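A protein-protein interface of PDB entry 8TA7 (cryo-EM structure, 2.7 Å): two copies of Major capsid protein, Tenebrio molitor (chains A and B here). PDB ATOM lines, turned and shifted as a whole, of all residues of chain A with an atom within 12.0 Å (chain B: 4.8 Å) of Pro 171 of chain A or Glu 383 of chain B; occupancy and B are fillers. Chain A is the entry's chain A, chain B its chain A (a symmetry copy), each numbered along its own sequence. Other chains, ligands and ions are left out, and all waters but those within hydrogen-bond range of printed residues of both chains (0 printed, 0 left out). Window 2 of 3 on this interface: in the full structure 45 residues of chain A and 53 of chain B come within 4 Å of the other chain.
Pro 171 of chain A touches four residues of chain B. Of chain A, only Pro 171 (3.5 Å) comes within 4 Å of Glu 383 of chain B. Val 281 of chain B touches none of the printed residues of chain A. No residue of chain A comes within 4 Å of Lys 283 of chain B. Of chain A, only Pro 171, Ile 172 and Gly 173 come within 4 Å of Asn 380 of chain B. Of the printed residues of chain A, Phe 381 of chain B touches Pro 171, Gly 173 and Leu 174. Ile 382 of chain B touches one residue of chain A. No residue of chain A comes within 4 Å of Phe 385 of chain B. Of the printed residues of chain B, Gly 173 of chain A touches Asn 380 (2.9 Å) and Phe 381 (3.5 Å). Of the printed residues of chain B, Leu 174 of chain A touches Phe 381 (3.7 Å). Val 176 of chain A touches none of the printed residues of chain B. The nearest printed residue of chain B that does not touch Pro 171 of chain A is Val 281 of chain B (6.0 Å). The nearest residue of chain A that does not touch Glu 383 of chain B is Ile 172 of chain A (7.7 Å).
Of the 6 printed residues of chain A, 4 touch a printed residue of chain B. Printed residues of chain A that touch a printed residue of chain B: Pro 171, Ile 172, Gly 173 and Leu 174. Hydrophobic or aromatic side chains of chain A that line the printed part of chain B: Pro 171, Ile 172 and Leu 174. Of the 10 printed residues of chain B, 4 touch a printed residue of chain A. Along chain B the printed residues that touch a printed residue of chain A span positions 380 to 383. Among the printed residues, 8 pairs touch across the chains. Among the printed residues, no Asp or Glu carboxylate lies within 4 Å of a Lys or Arg side-chain nitrogen of the other chain.
No position is printed for both chains. Of the 8 pairs that touch across the chains among the printed residues, none has its exchanged pair printed and touching as well.
The backbone carbonyl oxygen (O) of Asn 380 of chain B is in hydrogen-bond range of the backbone NH (N) of Ile 172 of chain A (3.0 Å). The backbone NH (N) of Gly 173 of chain A sits at hydrogen-bond distance from the backbone carbonyl oxygen (O) of Asn 380 of chain B (2.9 Å).
The backbone NH (N) of Val 281 of chain B lies within hydrogen-bond range of the backbone carbonyl oxygen (O) of Glu 383 of chain B, at 2.6 Å. The side-chain carboxylate of Glu 383 of chain B is in salt-bridge range of the side-chain amino group of Lys 283 of chain B, at 2.6 Å.
Among the printed residues, pairs that only touch across the chains: Pro 171 of chain A with Asn 380 of chain B, Pro 171 of chain A with Glu 383 of chain B, Gly 173 of chain A with Phe 381 of chain B, Leu 174 of chain A with Phe 381 of chain B, Pro 171 of chain A with Ile 382 of chain B and Pro 171 of chain A with Phe 381 of chain B.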
ATOM      1  N   PRO A 171      12.592 -14.719 -23.032  1.00  0.00           N
ATOM      2  CA  PRO A 171      12.779 -13.570 -23.923  1.00  0.00           C
ATOM      3  C   PRO A 171      12.792 -12.245 -23.169  1.00  0.00           C
ATOM      4  O   PRO A 171      11.734 -11.686 -22.879  1.00  0.00           O
ATOM      5  CB  PRO A 171      11.571 -13.650 -24.864  1.00  0.00           C
ATOM      6  CG  PRO A 171      11.084 -15.048 -24.755  1.00  0.00           C
ATOM      7  CD  PRO A 171      11.360 -15.457 -23.347  1.00  0.00           C
ATOM      8  N   ILE A 172      13.993 -11.752 -22.860  1.00  0.00           N
ATOM      9  CA  ILE A 172      14.133 -10.496 -22.135  1.00  0.00           C
ATOM     10  C   ILE A 172      13.740  -9.295 -22.985  1.00  0.00           C
ATOM     11  O   ILE A 172      13.256  -8.293 -22.448  1.00  0.00           O
ATOM     12  CB  ILE A 172      15.574 -10.361 -21.605  1.00  0.00           C
ATOM     13  CG1 ILE A 172      16.569 -10.284 -22.760  1.00  0.00           C
ATOM     14  CG2 ILE A 172      15.908 -11.533 -20.701  1.00  0.00           C
ATOM     15  CD1 ILE A 172      17.980 -10.001 -22.327  1.00  0.00           C
ATOM     16  N   GLY A 173      13.932  -9.366 -24.301  1.00  0.00           N
ATOM     17  CA  GLY A 173      13.534  -8.274 -25.164  1.00  0.00           C
ATOM     18  C   GLY A 173      14.599  -7.196 -25.296  1.00  0.00           C
ATOM     19  O   GLY A 173      15.778  -7.390 -24.992  1.00  0.00           O
ATOM     20  N   LEU A 174      14.154  -6.035 -25.776  1.00  0.00           N
ATOM     21  CA  LEU A 174      15.054  -4.905 -25.970  1.00  0.00           C
ATOM     22  C   LEU A 174      15.598  -4.371 -24.657  1.00  0.00           C
ATOM     23  O   LEU A 174      14.907  -4.341 -23.635  1.00  0.00           O
ATOM     24  CB  LEU A 174      14.350  -3.769 -26.707  1.00  0.00           C
ATOM     25  CG  LEU A 174      13.940  -4.007 -28.146  1.00  0.00           C
ATOM     26  CD1 LEU A 174      13.139  -2.831 -28.654  1.00  0.00           C
ATOM     27  CD2 LEU A 174      15.225  -4.144 -28.926  1.00  0.00           C
ATOM     28  N   HIS A 175      16.851  -3.932 -24.702  1.00  0.00           N
ATOM     29  CA  HIS A 175      17.399  -3.065 -23.670  1.00  0.00           C
ATOM     30  C   HIS A 175      16.993  -1.631 -23.979  1.00  0.00           C
ATOM     31  O   HIS A 175      17.574  -0.987 -24.857  1.00  0.00           O
ATOM     32  CB  HIS A 175      18.915  -3.199 -23.607  1.00  0.00           C
ATOM     33  CG  HIS A 175      19.541  -2.425 -22.491  1.00  0.00           C
ATOM     34  ND1 HIS A 175      20.866  -2.044 -22.503  1.00  0.00           N
ATOM     35  CD2 HIS A 175      19.028  -1.960 -21.328  1.00  0.00           C
ATOM     36  CE1 HIS A 175      21.138  -1.371 -21.400  1.00  0.00           C
ATOM     37  NE2 HIS A 175      20.040  -1.308 -20.668  1.00  0.00           N
ATOM     38  N   VAL A 176      15.980  -1.138 -23.275  1.00  0.00           N
ATOM     39  CA  VAL A 176      15.518   0.235 -23.408  1.00  0.00           C
ATOM     40  C   VAL A 176      15.790   0.945 -22.094  1.00  0.00           C
ATOM     41  O   VAL A 176      15.250   0.559 -21.053  1.00  0.00           O
ATOM     42  CB  VAL A 176      14.020   0.309 -23.766  1.00  0.00           C
ATOM     43  CG1 VAL A 176      13.580   1.760 -23.884  1.00  0.00           C
ATOM     44  CG2 VAL A 176      13.746  -0.438 -25.062  1.00  0.00           C
ATOM     45  N   LEU B 279      16.562 -26.611 -26.511  1.00  0.00           N
ATOM     46  CA  LEU B 279      15.432 -26.478 -27.421  1.00  0.00           C
ATOM     47  C   LEU B 279      15.064 -25.008 -27.572  1.00  0.00           C
ATOM     48  O   LEU B 279      14.686 -24.357 -26.596  1.00  0.00           O
ATOM     49  CB  LEU B 279      14.240 -27.275 -26.897  1.00  0.00           C
ATOM     50  CG  LEU B 279      12.933 -27.109 -27.661  1.00  0.00           C
ATOM     51  CD1 LEU B 279      12.957 -27.966 -28.893  1.00  0.00           C
ATOM     52  CD2 LEU B 279      11.768 -27.476 -26.777  1.00  0.00           C
ATOM     53  N   GLN B 280      15.157 -24.497 -28.796  1.00  0.00           N
ATOM     54  CA  GLN B 280      14.843 -23.109 -29.103  1.00  0.00           C
ATOM     55  C   GLN B 280      13.419 -23.004 -29.633  1.00  0.00           C
ATOM     56  O   GLN B 280      13.030 -23.749 -30.540  1.00  0.00           O
ATOM     57  CB  GLN B 280      15.820 -22.547 -30.135  1.00  0.00           C
ATOM     58  CG  GLN B 280      17.281 -22.751 -29.805  1.00  0.00           C
ATOM     59  CD  GLN B 280      18.186 -21.985 -30.744  1.00  0.00           C
ATOM     60  OE1 GLN B 280      18.390 -22.384 -31.890  1.00  0.00           O
ATOM     61  NE2 GLN B 280      18.729 -20.874 -30.269  1.00  0.00           N
ATOM     62  N   VAL B 281      12.651 -22.075 -29.067  1.00  0.00           N
ATOM     63  CA  VAL B 281      11.282 -21.796 -29.489  1.00  0.00           C
ATOM     64  C   VAL B 281      11.170 -20.295 -29.721  1.00  0.00           C
ATOM     65  O   VAL B 281      11.367 -19.504 -28.793  1.00  0.00           O
ATOM     66  CB  VAL B 281      10.249 -22.264 -28.457  1.00  0.00           C
ATOM     67  CG1 VAL B 281       8.873 -21.737 -28.815  1.00  0.00           C
ATOM     68  CG2 VAL B 281      10.234 -23.777 -28.371  1.00  0.00           C
ATOM     69  N   LYS B 283       8.548 -17.413 -31.044  1.00  0.00           N
ATOM     70  CA  LYS B 283       7.178 -17.040 -31.370  1.00  0.00           C
ATOM     71  C   LYS B 283       7.134 -15.556 -31.706  1.00  0.00           C
ATOM     72  O   LYS B 283       7.618 -14.726 -30.930  1.00  0.00           O
ATOM     73  CB  LYS B 283       6.228 -17.354 -30.215  1.00  0.00           C
ATOM     74  CG  LYS B 283       6.083 -18.832 -29.916  1.00  0.00           C
ATOM     75  CD  LYS B 283       5.050 -19.074 -28.833  1.00  0.00           C
ATOM     76  CE  LYS B 283       5.551 -18.623 -27.477  1.00  0.00           C
ATOM     77  NZ  LYS B 283       6.684 -19.463 -27.011  1.00  0.00           N
ATOM     78  N   ASN B 380      17.732 -12.734 -27.571  1.00  0.00           N
ATOM     79  CA  ASN B 380      17.016 -12.092 -26.478  1.00  0.00           C
ATOM     80  C   ASN B 380      15.508 -12.176 -26.652  1.00  0.00           C
ATOM     81  O   ASN B 380      14.768 -11.792 -25.740  1.00  0.00           O
ATOM     82  CB  ASN B 380      17.442 -10.630 -26.361  1.00  0.00           C
ATOM     83  CG  ASN B 380      18.818 -10.470 -25.752  1.00  0.00           C
ATOM     84  OD1 ASN B 380      19.379 -11.416 -25.205  1.00  0.00           O
ATOM     85  ND2 ASN B 380      19.371  -9.270 -25.850  1.00  0.00           N
ATOM     86  N   PHE B 381      15.038 -12.659 -27.801  1.00  0.00           N
ATOM     87  CA  PHE B 381      13.619 -12.711 -28.108  1.00  0.00           C
ATOM     88  C   PHE B 381      13.092 -14.122 -28.318  1.00  0.00           C
ATOM     89  O   PHE B 381      11.949 -14.276 -28.760  1.00  0.00           O
ATOM     90  CB  PHE B 381      13.317 -11.866 -29.355  1.00  0.00           C
ATOM     91  CG  PHE B 381      13.829 -10.460 -29.264  1.00  0.00           C
ATOM     92  CD1 PHE B 381      15.118 -10.150 -29.661  1.00  0.00           C
ATOM     93  CD2 PHE B 381      13.026  -9.448 -28.770  1.00  0.00           C
ATOM     94  CE1 PHE B 381      15.593  -8.863 -29.568  1.00  0.00           C
ATOM     95  CE2 PHE B 381      13.496  -8.158 -28.679  1.00  0.00           C
ATOM     96  CZ  PHE B 381      14.781  -7.865 -29.077  1.00  0.00           C
ATOM     97  N   ILE B 382      13.883 -15.145 -28.024  1.00  0.00           N
ATOM     98  CA  ILE B 382      13.468 -16.530 -28.199  1.00  0.00           C
ATOM     99  C   ILE B 382      13.486 -17.229 -26.850  1.00  0.00           C
ATOM    100  O   ILE B 382      14.169 -16.806 -25.911  1.00  0.00           O
ATOM    101  CB  ILE B 382      14.367 -17.264 -29.215  1.00  0.00           C
ATOM    102  CG1 ILE B 382      15.785 -17.405 -28.669  1.00  0.00           C
ATOM    103  CG2 ILE B 382      14.386 -16.526 -30.539  1.00  0.00           C
ATOM    104  CD1 ILE B 382      16.693 -18.235 -29.538  1.00  0.00           C
ATOM    105  N   GLU B 383      12.718 -18.307 -26.750  1.00  0.00           N
ATOM    106  CA  GLU B 383      12.730 -19.167 -25.576  1.00  0.00           C
ATOM    107  C   GLU B 383      13.633 -20.363 -25.829  1.00  0.00           C
ATOM    108  O   GLU B 383      13.572 -20.988 -26.892  1.00  0.00           O
ATOM    109  CB  GLU B 383      11.320 -19.645 -25.235  1.00  0.00           C
ATOM    110  CG  GLU B 383      10.440 -18.589 -24.614  1.00  0.00           C
ATOM    111  CD  GLU B 383       9.004 -18.675 -25.085  1.00  0.00           C
ATOM    112  OE1 GLU B 383       8.395 -17.614 -25.330  1.00  0.00           O
ATOM    113  OE2 GLU B 383       8.486 -19.805 -25.214  1.00  0.00           O
ATOM    114  N   GLU B 384      14.472 -20.682 -24.849  1.00  0.00           N
ATOM    115  CA  GLU B 384      15.357 -21.827 -24.966  1.00  0.00           C
ATOM    116  C   GLU B 384      15.182 -22.725 -23.753  1.00  0.00           C
ATOM    117  O   GLU B 384      15.309 -22.274 -22.612  1.00  0.00           O
ATOM    118  CB  GLU B 384      16.818 -21.396 -25.112  1.00  0.00           C
ATOM    119  CG  GLU B 384      17.679 -22.411 -25.839  1.00  0.00           C
ATOM    120  CD  GLU B 384      18.943 -21.802 -26.402  1.00  0.00           C
ATOM    121  OE1 GLU B 384      18.840 -20.827 -27.175  1.00  0.00           O
ATOM    122  OE2 GLU B 384      20.041 -22.299 -26.076  1.00  0.00           O
ATOM    123  N   PHE B 385      14.895 -23.998 -24.011  1.00  0.00           N
ATOM    124  CA  PHE B 385      14.576 -24.964 -22.973  1.00  0.00           C
ATOM    125  C   PHE B 385      15.643 -26.047 -22.936  1.00  0.00           C
ATOM    126  O   PHE B 385      16.470 -26.166 -23.843  1.00  0.00           O
ATOM    127  CB  PHE B 385      13.203 -25.610 -23.211  1.00  0.00           C
ATOM    128  CG  PHE B 385      12.083 -24.627 -23.353  1.00  0.00           C
ATOM    129  CD1 PHE B 385      11.415 -24.148 -22.240  1.00  0.00           C
ATOM    130  CD2 PHE B 385      11.694 -24.180 -24.605  1.00  0.00           C
ATOM    131  CE1 PHE B 385      10.381 -23.244 -22.371  1.00  0.00           C
ATOM    132  CE2 PHE B 385      10.662 -23.275 -24.743  1.00  0.00           C
ATOM    133  CZ  PHE B 385      10.002 -22.807 -23.625  1.00  0.00           C
